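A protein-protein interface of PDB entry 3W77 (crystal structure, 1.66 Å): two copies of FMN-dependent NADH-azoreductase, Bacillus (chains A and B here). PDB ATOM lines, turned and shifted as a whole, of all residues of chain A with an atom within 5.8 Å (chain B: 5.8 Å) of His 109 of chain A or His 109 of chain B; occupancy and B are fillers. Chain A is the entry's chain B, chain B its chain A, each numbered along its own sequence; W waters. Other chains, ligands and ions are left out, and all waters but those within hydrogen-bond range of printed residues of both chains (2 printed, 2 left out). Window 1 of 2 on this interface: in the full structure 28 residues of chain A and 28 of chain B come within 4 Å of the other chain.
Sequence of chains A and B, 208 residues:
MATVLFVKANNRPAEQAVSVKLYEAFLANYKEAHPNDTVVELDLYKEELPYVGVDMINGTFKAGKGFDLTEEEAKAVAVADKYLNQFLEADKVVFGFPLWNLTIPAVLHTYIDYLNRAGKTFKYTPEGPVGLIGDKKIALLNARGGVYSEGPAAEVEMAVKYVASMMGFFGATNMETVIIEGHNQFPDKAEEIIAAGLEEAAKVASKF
The backbone carbonyl oxygen of Ile 104 of chain B sits close to a ring nitrogen (NE2) of His 109 of chain A, 3.1 Å away. A ring nitrogen (NE2) of His 109 of chain B lies close to the backbone carbonyl oxygen (O) of Ile 104 of chain A (3.1 Å). ND1 of His 109 of chain B is in hydrogen-bond range of ND1 of His 109 of chain A (2.8 Å).
Hydrophobic or aromatic side chains of chain A that line the printed part of chain B: Ala 106, His 109 and Tyr 162. Of the 14 printed residues of chain B, 7 touch a printed residue of chain A. Hydrophobic or aromatic side chains of chain B that line the printed part of chain A: Ala 106, His 109 and Tyr 162. Among the printed residues, no Asp or Glu carboxylate lies within 4 Å of a Lys or Arg side-chain nitrogen of the other chain.
Of the printed residues of chain B, Thr 103 of chain A touches His 109 (3.4 Å) and Tyr 162 (3.5 Å). Leu 108 of chain A touches none of the printed residues of chain B. Of the printed residues of chain B, His 109 of chain A touches Thr 103, Ile 104, Pro 105, Ala 106 and His 109. Of the printed residues of chain B, Tyr 162 of chain A touches Thr 103 (3.5 Å). Printed residues of chain A within 4 Å of Thr 103 of chain B: His 109 (3.3 Å) and Tyr 162 (3.5 Å). Of the printed residues of chain A, His 109 of chain B touches Thr 103, Ile 104, Pro 105, Ala 106 and His 109. The nearest residue of chain B that does not touch His 109 of chain A is Trp 100 of chain B (5.1 Å). The nearest residue of chain A that does not touch His 109 of chain B is Trp 100 of chain A (5.1 Å).
Thr 103 of chain A touches Tyr 162 of chain B, and with the chains exchanged Tyr 162 of chain A touches Thr 103 of chain B. Pro 105 of chain A touches His 109 of chain B, and with the chains exchanged His 109 of chain A touches Pro 105 of chain B. Ala 106 of chain A touches His 109 of chain B, and with the chains exchanged His 109 of chain A touches Ala 106 of chain B. His 109 of chain A touches its own counterpart, His 109 of chain B. Of the 13 pairs that touch across the chains among the printed residues, 13 have their exchanged pair printed and touching as well.
Water W1 bridges the side-chain carboxylate (OD2) of Asp 113 of chain A (2.6 Å) and the backbone NH (N) of Ala 106 of chain B (2.9 Å). Water W2 lies within hydrogen-bond range of the side-chain carboxylate of Asp 113 of chain B and the backbone NH of Ala 106 of chain A.
Thr 103 of chain A touches His 109 of chain B. Thr 103 of chain A touches Tyr 162 of chain B. His 109 of chain B touches Pro 105 of chain A. Ala 106 of chain A touches His 109 of chain B. Ala 106 of chain A touches Thr 110 of chain B (CB to OG1, 3.4 Å). CG2 of Thr 103 of chain B touches NE2 of His 109 of chain A, at 3.3 Å. Pro 105 of chain B touches His 109 of chain A. His 109 of chain A touches Ala 106 of chain B. Thr 110 of chain A touches Ala 106 of chain B (OG1 to CB, 3.4 Å). Thr 103 of chain B touches Tyr 162 of chain A.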
ATOM      1  N   TRP A 100     -15.240  15.469  12.328  1.00  0.00           N
ATOM      2  CA  TRP A 100     -16.633  15.888  12.230  1.00  0.00           C
ATOM      3  C   TRP A 100     -16.632  17.192  11.507  1.00  0.00           C
ATOM      4  O   TRP A 100     -15.946  18.117  11.912  1.00  0.00           O
ATOM      5  CB  TRP A 100     -17.273  16.143  13.618  1.00  0.00           C
ATOM      6  CG  TRP A 100     -17.529  14.929  14.506  1.00  0.00           C
ATOM      7  CD1 TRP A 100     -17.636  13.587  14.155  1.00  0.00           C
ATOM      8  CD2 TRP A 100     -17.853  14.985  15.942  1.00  0.00           C
ATOM      9  NE1 TRP A 100     -17.937  12.817  15.267  1.00  0.00           N
ATOM     10  CE2 TRP A 100     -18.073  13.601  16.376  1.00  0.00           C
ATOM     11  CE3 TRP A 100     -17.923  16.010  16.874  1.00  0.00           C
ATOM     12  CZ2 TRP A 100     -18.357  13.284  17.701  1.00  0.00           C
ATOM     13  CZ3 TRP A 100     -18.215  15.686  18.216  1.00  0.00           C
ATOM     14  CH2 TRP A 100     -18.433  14.360  18.613  1.00  0.00           C
ATOM     15  N   THR A 103     -13.224  18.565  10.540  1.00  0.00           N
ATOM     16  CA  THR A 103     -12.180  18.986  11.531  1.00  0.00           C
ATOM     17  C   THR A 103     -12.341  18.238  12.853  1.00  0.00           C
ATOM     18  O   THR A 103     -13.096  17.261  12.935  1.00  0.00           O
ATOM     19  CB  THR A 103     -12.193  20.528  11.703  1.00  0.00           C
ATOM     20  OG1 THR A 103     -11.066  20.990  12.481  1.00  0.00           O
ATOM     21  CG2 THR A 103     -13.536  21.037  12.309  1.00  0.00           C
ATOM     22  N   ILE A 104     -11.627  18.696  13.878  1.00  0.00           N
ATOM     23  CA  ILE A 104     -11.747  18.080  15.204  1.00  0.00           C
ATOM     24  C   ILE A 104     -13.006  18.598  15.903  1.00  0.00           C
ATOM     25  O   ILE A 104     -13.504  19.658  15.559  1.00  0.00           O
ATOM     26  CB  ILE A 104     -10.503  18.401  16.070  1.00  0.00           C
ATOM     27  CG1 ILE A 104     -10.299  19.916  16.189  1.00  0.00           C
ATOM     28  CG2 ILE A 104      -9.259  17.719  15.498  1.00  0.00           C
ATOM     29  CD1 ILE A 104      -9.136  20.320  17.093  1.00  0.00           C
ATOM     30  N   PRO A 105     -13.518  17.851  16.909  1.00  0.00           N
ATOM     31  CA  PRO A 105     -14.571  18.433  17.763  1.00  0.00           C
ATOM     32  C   PRO A 105     -14.157  19.789  18.319  1.00  0.00           C
ATOM     33  O   PRO A 105     -12.968  20.002  18.713  1.00  0.00           O
ATOM     34  CB  PRO A 105     -14.707  17.400  18.902  1.00  0.00           C
ATOM     35  CG  PRO A 105     -14.277  16.102  18.251  1.00  0.00           C
ATOM     36  CD  PRO A 105     -13.101  16.499  17.375  1.00  0.00           C
ATOM     37  N   ALA A 106     -15.122  20.716  18.377  1.00  0.00           N
ATOM     38  CA  ALA A 106     -14.819  22.016  18.971  1.00  0.00           C
ATOM     39  C   ALA A 106     -14.310  21.910  20.420  1.00  0.00           C
ATOM     40  O   ALA A 106     -13.522  22.757  20.841  1.00  0.00           O
ATOM     41  CB  ALA A 106     -16.035  22.951  18.887  1.00  0.00           C
ATOM     42  N   VAL A 107     -14.733  20.879  21.186  1.00  0.00           N
ATOM     43  CA  VAL A 107     -14.151  20.730  22.545  1.00  0.00           C
ATOM     44  C   VAL A 107     -12.616  20.596  22.502  1.00  0.00           C
ATOM     45  O   VAL A 107     -11.880  21.156  23.342  1.00  0.00           O
ATOM     46  CB  VAL A 107     -14.751  19.574  23.375  1.00  0.00           C
ATOM     47  CG1 VAL A 107     -16.225  19.807  23.659  1.00  0.00           C
ATOM     48  CG2 VAL A 107     -14.573  18.224  22.736  1.00  0.00           C
ATOM     49  N   LEU A 108     -12.118  19.852  21.521  1.00  0.00           N
ATOM     50  CA  LEU A 108     -10.652  19.692  21.403  1.00  0.00           C
ATOM     51  C   LEU A 108      -9.957  20.943  20.856  1.00  0.00           C
ATOM     52  O   LEU A 108      -8.833  21.262  21.223  1.00  0.00           O
ATOM     53  CB  LEU A 108     -10.346  18.425  20.557  1.00  0.00           C
ATOM     54  CG  LEU A 108      -8.887  18.126  20.310  1.00  0.00           C
ATOM     55  CD1 LEU A 108      -8.122  17.879  21.589  1.00  0.00           C
ATOM     56  CD2 LEU A 108      -8.735  16.905  19.388  1.00  0.00           C
ATOM     57  N   HIS A 109     -10.651  21.669  19.986  1.00  0.00           N
ATOM     58  CA  HIS A 109     -10.181  22.965  19.476  1.00  0.00           C
ATOM     59  C   HIS A 109      -9.968  23.909  20.675  1.00  0.00           C
ATOM     60  O   HIS A 109      -8.903  24.491  20.822  1.00  0.00           O
ATOM     61  CB  HIS A 109     -11.270  23.444  18.492  1.00  0.00           C
ATOM     62  CG  HIS A 109     -11.038  24.780  17.853  1.00  0.00           C
ATOM     63  ND1 HIS A 109     -11.867  25.244  16.872  1.00  0.00           N
ATOM     64  CD2 HIS A 109     -10.105  25.777  18.092  1.00  0.00           C
ATOM     65  CE1 HIS A 109     -11.472  26.491  16.513  1.00  0.00           C
ATOM     66  NE2 HIS A 109     -10.390  26.811  17.248  1.00  0.00           N
ATOM     67  N   THR A 110     -10.949  24.005  21.579  1.00  0.00           N
ATOM     68  CA  THR A 110     -10.752  24.848  22.791  1.00  0.00           C
ATOM     69  C   THR A 110      -9.585  24.336  23.638  1.00  0.00           C
ATOM     70  O   THR A 110      -8.760  25.126  24.098  1.00  0.00           O
ATOM     71  CB  THR A 110     -12.071  24.951  23.606  1.00  0.00           C
ATOM     72  OG1 THR A 110     -13.016  25.742  22.845  1.00  0.00           O
ATOM     73  CG2 THR A 110     -11.800  25.661  24.965  1.00  0.00           C
ATOM     74  N   TYR A 111      -9.494  23.018  23.843  1.00  0.00           N
ATOM     75  CA  TYR A 111      -8.389  22.480  24.666  1.00  0.00           C
ATOM     76  C   TYR A 111      -7.022  22.876  24.061  1.00  0.00           C
ATOM     77  O   TYR A 111      -6.090  23.281  24.797  1.00  0.00           O
ATOM     78  CB  TYR A 111      -8.509  20.964  24.755  1.00  0.00           C
ATOM     79  CG  TYR A 111      -7.374  20.282  25.484  1.00  0.00           C
ATOM     80  CD1 TYR A 111      -7.335  20.265  26.890  1.00  0.00           C
ATOM     81  CD2 TYR A 111      -6.343  19.630  24.762  1.00  0.00           C
ATOM     82  CE1 TYR A 111      -6.303  19.613  27.584  1.00  0.00           C
ATOM     83  CE2 TYR A 111      -5.298  18.992  25.442  1.00  0.00           C
ATOM     84  CZ  TYR A 111      -5.295  18.977  26.832  1.00  0.00           C
ATOM     85  OH  TYR A 111      -4.283  18.321  27.491  1.00  0.00           O
ATOM     86  N   ILE A 112      -6.874  22.717  22.740  1.00  0.00           N
ATOM     87  CA  ILE A 112      -5.595  23.069  22.115  1.00  0.00           C
ATOM     88  C   ILE A 112      -5.341  24.582  22.192  1.00  0.00           C
ATOM     89  O   ILE A 112      -4.176  25.024  22.409  1.00  0.00           O
ATOM     90  CB  ILE A 112      -5.488  22.504  20.672  1.00  0.00           C
ATOM     91  CG1 ILE A 112      -5.586  20.983  20.732  1.00  0.00           C
ATOM     92  CG2 ILE A 112      -4.201  22.986  20.009  1.00  0.00           C
ATOM     93  CD1 ILE A 112      -5.739  20.348  19.347  1.00  0.00           C
ATOM     94  N   ASP A 113      -6.414  25.374  22.140  1.00  0.00           N
ATOM     95  CA  ASP A 113      -6.251  26.837  22.335  1.00  0.00           C
ATOM     96  C   ASP A 113      -5.583  27.118  23.712  1.00  0.00           C
ATOM     97  O   ASP A 113      -4.746  28.040  23.836  1.00  0.00           O
ATOM     98  CB  ASP A 113      -7.598  27.592  22.316  1.00  0.00           C
ATOM     99  CG  ASP A 113      -8.273  27.701  20.931  1.00  0.00           C
ATOM    100  OD1 ASP A 113      -7.599  27.707  19.886  1.00  0.00           O
ATOM    101  OD2 ASP A 113      -9.531  27.865  20.927  1.00  0.00           O
ATOM    102  N   TYR A 114      -5.997  26.385  24.755  1.00  0.00           N
ATOM    103  CA  TYR A 114      -5.428  26.576  26.112  1.00  0.00           C
ATOM    104  C   TYR A 114      -3.952  26.222  26.156  1.00  0.00           C
ATOM    105  O   TYR A 114      -3.221  26.718  27.027  1.00  0.00           O
ATOM    106  CB  TYR A 114      -6.104  25.677  27.148  1.00  0.00           C
ATOM    107  CG  TYR A 114      -7.570  25.894  27.441  1.00  0.00           C
ATOM    108  CD1 TYR A 114      -8.253  27.056  27.045  1.00  0.00           C
ATOM    109  CD2 TYR A 114      -8.275  24.923  28.141  1.00  0.00           C
ATOM    110  CE1 TYR A 114      -9.609  27.233  27.337  1.00  0.00           C
ATOM    111  CE2 TYR A 114      -9.623  25.082  28.439  1.00  0.00           C
ATOM    112  CZ  TYR A 114     -10.284  26.236  28.031  1.00  0.00           C
ATOM    113  OH  TYR A 114     -11.634  26.369  28.330  1.00  0.00           O
ATOM    114  N   TYR A 162      -4.916  19.580  11.502  1.00  0.00           N
ATOM    115  CA  TYR A 162      -4.951  20.670  12.502  1.00  0.00           C
ATOM    116  C   TYR A 162      -4.128  20.277  13.743  1.00  0.00           C
ATOM    117  O   TYR A 162      -3.262  21.038  14.196  1.00  0.00           O
ATOM    118  CB  TYR A 162      -6.402  21.039  12.876  1.00  0.00           C
ATOM    119  CG  TYR A 162      -6.385  22.218  13.824  1.00  0.00           C
ATOM    120  CD1 TYR A 162      -6.402  22.019  15.214  1.00  0.00           C
ATOM    121  CD2 TYR A 162      -6.233  23.511  13.322  1.00  0.00           C
ATOM    122  CE1 TYR A 162      -6.311  23.098  16.088  1.00  0.00           C
ATOM    123  CE2 TYR A 162      -6.131  24.595  14.181  1.00  0.00           C
ATOM    124  CZ  TYR A 162      -6.149  24.379  15.553  1.00  0.00           C
ATOM    125  OH  TYR A 162      -6.056  25.476  16.378  1.00  0.00           O
ATOM    126  N   TRP B 100      -7.094  32.613  14.564  1.00  0.00           N
ATOM    127  CA  TRP B 100      -6.433  32.345  15.828  1.00  0.00           C
ATOM    128  C   TRP B 100      -5.991  30.914  15.788  1.00  0.00           C
ATOM    129  O   TRP B 100      -6.823  30.008  15.557  1.00  0.00           O
ATOM    130  CB  TRP B 100      -7.383  32.530  17.000  1.00  0.00           C
ATOM    131  CG  TRP B 100      -7.823  33.958  17.327  1.00  0.00           C
ATOM    132  CD1 TRP B 100      -7.251  35.174  16.931  1.00  0.00           C
ATOM    133  CD2 TRP B 100      -8.908  34.331  18.267  1.00  0.00           C
ATOM    134  NE1 TRP B 100      -7.918  36.240  17.528  1.00  0.00           N
ATOM    135  CE2 TRP B 100      -8.930  35.793  18.316  1.00  0.00           C
ATOM    136  CE3 TRP B 100      -9.841  33.607  18.995  1.00  0.00           C
ATOM    137  CZ2 TRP B 100      -9.878  36.488  19.083  1.00  0.00           C
ATOM    138  CZ3 TRP B 100     -10.786  34.312  19.766  1.00  0.00           C
ATOM    139  CH2 TRP B 100     -10.795  35.714  19.793  1.00  0.00           C
ATOM    140  N   THR B 103      -6.888  28.849  12.731  1.00  0.00           N
ATOM    141  CA  THR B 103      -8.299  28.570  12.371  1.00  0.00           C
ATOM    142  C   THR B 103      -9.266  29.637  12.882  1.00  0.00           C
ATOM    143  O   THR B 103      -8.845  30.716  13.276  1.00  0.00           O
ATOM    144  CB  THR B 103      -8.694  27.115  12.803  1.00  0.00           C
ATOM    145  OG1 THR B 103      -9.942  26.740  12.202  1.00  0.00           O
ATOM    146  CG2 THR B 103      -8.739  26.967  14.352  1.00  0.00           C
ATOM    147  N   ILE B 104     -10.571  29.376  12.763  1.00  0.00           N
ATOM    148  CA  ILE B 104     -11.580  30.283  13.298  1.00  0.00           C
ATOM    149  C   ILE B 104     -11.716  30.151  14.831  1.00  0.00           C
ATOM    150  O   ILE B 104     -11.315  29.143  15.407  1.00  0.00           O
ATOM    151  CB  ILE B 104     -12.979  29.975  12.680  1.00  0.00           C
ATOM    152  CG1 ILE B 104     -13.343  28.481  12.850  1.00  0.00           C
ATOM    153  CG2 ILE B 104     -12.980  30.374  11.195  1.00  0.00           C
ATOM    154  CD1 ILE B 104     -14.756  28.152  12.341  1.00  0.00           C
ATOM    155  N   PRO B 105     -12.303  31.160  15.501  1.00  0.00           N
ATOM    156  CA  PRO B 105     -12.601  30.958  16.935  1.00  0.00           C
ATOM    157  C   PRO B 105     -13.495  29.742  17.155  1.00  0.00           C
ATOM    158  O   PRO B 105     -14.398  29.476  16.354  1.00  0.00           O
ATOM    159  CB  PRO B 105     -13.298  32.268  17.343  1.00  0.00           C
ATOM    160  CG  PRO B 105     -12.741  33.286  16.361  1.00  0.00           C
ATOM    161  CD  PRO B 105     -12.608  32.536  15.048  1.00  0.00           C
ATOM    162  N   ALA B 106     -13.234  28.999  18.236  1.00  0.00           N
ATOM    163  CA  ALA B 106     -14.055  27.805  18.530  1.00  0.00           C
ATOM    164  C   ALA B 106     -15.539  28.178  18.693  1.00  0.00           C
ATOM    165  O   ALA B 106     -16.398  27.352  18.353  1.00  0.00           O
ATOM    166  CB  ALA B 106     -13.512  27.063  19.765  1.00  0.00           C
ATOM    167  N   VAL B 107     -15.860  29.410  19.127  1.00  0.00           N
ATOM    168  CA  VAL B 107     -17.299  29.793  19.127  1.00  0.00           C
ATOM    169  C   VAL B 107     -17.964  29.700  17.737  1.00  0.00           C
ATOM    170  O   VAL B 107     -19.119  29.217  17.624  1.00  0.00           O
ATOM    171  CB  VAL B 107     -17.583  31.189  19.738  1.00  0.00           C
ATOM    172  CG1 VAL B 107     -17.254  31.229  21.213  1.00  0.00           C
ATOM    173  CG2 VAL B 107     -16.826  32.319  19.050  1.00  0.00           C
ATOM    174  N   LEU B 108     -17.225  30.107  16.691  1.00  0.00           N
ATOM    175  CA  LEU B 108     -17.744  30.058  15.333  1.00  0.00           C
ATOM    176  C   LEU B 108     -17.774  28.622  14.796  1.00  0.00           C
ATOM    177  O   LEU B 108     -18.683  28.269  14.029  1.00  0.00           O
ATOM    178  CB  LEU B 108     -16.962  31.031  14.408  1.00  0.00           C
ATOM    179  CG  LEU B 108     -17.500  31.075  12.959  1.00  0.00           C
ATOM    180  CD1 LEU B 108     -18.974  31.484  12.804  1.00  0.00           C
ATOM    181  CD2 LEU B 108     -16.619  32.040  12.179  1.00  0.00           C
ATOM    182  N   HIS B 109     -16.814  27.803  15.234  1.00  0.00           N
ATOM    183  CA  HIS B 109     -16.760  26.369  14.889  1.00  0.00           C
ATOM    184  C   HIS B 109     -18.070  25.709  15.398  1.00  0.00           C
ATOM    185  O   HIS B 109     -18.786  25.030  14.644  1.00  0.00           O
ATOM    186  CB  HIS B 109     -15.502  25.826  15.577  1.00  0.00           C
ATOM    187  CG  HIS B 109     -15.234  24.356  15.377  1.00  0.00           C
ATOM    188  ND1 HIS B 109     -14.061  23.795  15.792  1.00  0.00           N
ATOM    189  CD2 HIS B 109     -15.993  23.327  14.837  1.00  0.00           C
ATOM    190  CE1 HIS B 109     -14.076  22.474  15.533  1.00  0.00           C
ATOM    191  NE2 HIS B 109     -15.255  22.171  14.970  1.00  0.00           N
ATOM    192  N   THR B 110     -18.409  25.931  16.668  1.00  0.00           N
ATOM    193  CA  THR B 110     -19.690  25.372  17.216  1.00  0.00           C
ATOM    194  C   THR B 110     -20.911  25.894  16.472  1.00  0.00           C
ATOM    195  O   THR B 110     -21.817  25.124  16.150  1.00  0.00           O
ATOM    196  CB  THR B 110     -19.812  25.670  18.729  1.00  0.00           C
ATOM    197  OG1 THR B 110     -18.778  24.923  19.397  1.00  0.00           O
ATOM    198  CG2 THR B 110     -21.214  25.273  19.288  1.00  0.00           C
ATOM    199  N   TYR B 111     -20.934  27.206  16.210  1.00  0.00           N
ATOM    200  CA  TYR B 111     -22.037  27.808  15.425  1.00  0.00           C
ATOM    201  C   TYR B 111     -22.217  27.100  14.069  1.00  0.00           C
ATOM    202  O   TYR B 111     -23.351  26.709  13.687  1.00  0.00           O
ATOM    203  CB  TYR B 111     -21.799  29.316  15.257  1.00  0.00           C
ATOM    204  CG  TYR B 111     -22.905  29.977  14.431  1.00  0.00           C
ATOM    205  CD1 TYR B 111     -24.166  30.291  15.015  1.00  0.00           C
ATOM    206  CD2 TYR B 111     -22.680  30.339  13.092  1.00  0.00           C
ATOM    207  CE1 TYR B 111     -25.158  30.899  14.261  1.00  0.00           C
ATOM    208  CE2 TYR B 111     -23.674  30.936  12.328  1.00  0.00           C
ATOM    209  CZ  TYR B 111     -24.906  31.220  12.910  1.00  0.00           C
ATOM    210  OH  TYR B 111     -25.890  31.823  12.162  1.00  0.00           O
ATOM    211  N   ILE B 112     -21.125  26.900  13.332  1.00  0.00           N
ATOM    212  CA  ILE B 112     -21.218  26.244  12.029  1.00  0.00           C
ATOM    213  C   ILE B 112     -21.653  24.769  12.158  1.00  0.00           C
ATOM    214  O   ILE B 112     -22.471  24.294  11.342  1.00  0.00           O
ATOM    215  CB  ILE B 112     -19.914  26.451  11.212  1.00  0.00           C
ATOM    216  CG1 ILE B 112     -19.730  27.969  10.969  1.00  0.00           C
ATOM    217  CG2 ILE B 112     -19.952  25.638   9.891  1.00  0.00           C
ATOM    218  CD1 ILE B 112     -18.362  28.346  10.352  1.00  0.00           C
ATOM    219  N   ASP B 113     -21.207  24.116  13.236  1.00  0.00           N
ATOM    220  CA  ASP B 113     -21.676  22.731  13.534  1.00  0.00           C
ATOM    221  C   ASP B 113     -23.209  22.693  13.589  1.00  0.00           C
ATOM    222  O   ASP B 113     -23.852  21.786  13.040  1.00  0.00           O
ATOM    223  CB  ASP B 113     -21.183  22.212  14.892  1.00  0.00           C
ATOM    224  CG  ASP B 113     -19.690  21.886  14.945  1.00  0.00           C
ATOM    225  OD1 ASP B 113     -19.027  21.537  13.924  1.00  0.00           O
ATOM    226  OD2 ASP B 113     -19.170  21.888  16.090  1.00  0.00           O
ATOM    227  N   TYR B 114     -23.802  23.696  14.223  1.00  0.00           N
ATOM    228  CA  TYR B 114     -25.267  23.739  14.371  1.00  0.00           C
ATOM    229  C   TYR B 114     -25.963  23.895  13.021  1.00  0.00           C
ATOM    230  O   TYR B 114     -27.114  23.474  12.872  1.00  0.00           O
ATOM    231  CB  TYR B 114     -25.709  24.908  15.251  1.00  0.00           C
ATOM    232  CG  TYR B 114     -25.297  24.958  16.695  1.00  0.00           C
ATOM    233  CD1 TYR B 114     -24.810  23.843  17.383  1.00  0.00           C
ATOM    234  CD2 TYR B 114     -25.458  26.159  17.410  1.00  0.00           C
ATOM    235  CE1 TYR B 114     -24.461  23.943  18.729  1.00  0.00           C
ATOM    236  CE2 TYR B 114     -25.129  26.254  18.745  1.00  0.00           C
ATOM    237  CZ  TYR B 114     -24.638  25.136  19.399  1.00  0.00           C
ATOM    238  OH  TYR B 114     -24.283  25.224  20.730  1.00  0.00           O
ATOM    239  N   TYR B 162     -11.808  27.004   6.091  1.00  0.00           N
ATOM    240  CA  TYR B 162     -12.803  26.190   6.795  1.00  0.00           C
ATOM    241  C   TYR B 162     -14.243  26.695   6.493  1.00  0.00           C
ATOM    242  O   TYR B 162     -15.130  25.925   6.083  1.00  0.00           O
ATOM    243  CB  TYR B 162     -12.541  26.144   8.328  1.00  0.00           C
ATOM    244  CG  TYR B 162     -13.530  25.212   8.962  1.00  0.00           C
ATOM    245  CD1 TYR B 162     -13.334  23.819   8.870  1.00  0.00           C
ATOM    246  CD2 TYR B 162     -14.709  25.700   9.576  1.00  0.00           C
ATOM    247  CE1 TYR B 162     -14.278  22.934   9.402  1.00  0.00           C
ATOM    248  CE2 TYR B 162     -15.665  24.809  10.107  1.00  0.00           C
ATOM    249  CZ  TYR B 162     -15.439  23.442  10.013  1.00  0.00           C
ATOM    250  OH  TYR B 162     -16.369  22.544  10.487  1.00  0.00           O
HETATM  251  O   HOH W   1     -10.695  29.681  19.409  1.00  0.00           O
HETATM  252  O   HOH W   2     -17.450  19.990  16.834  1.00  0.00           O
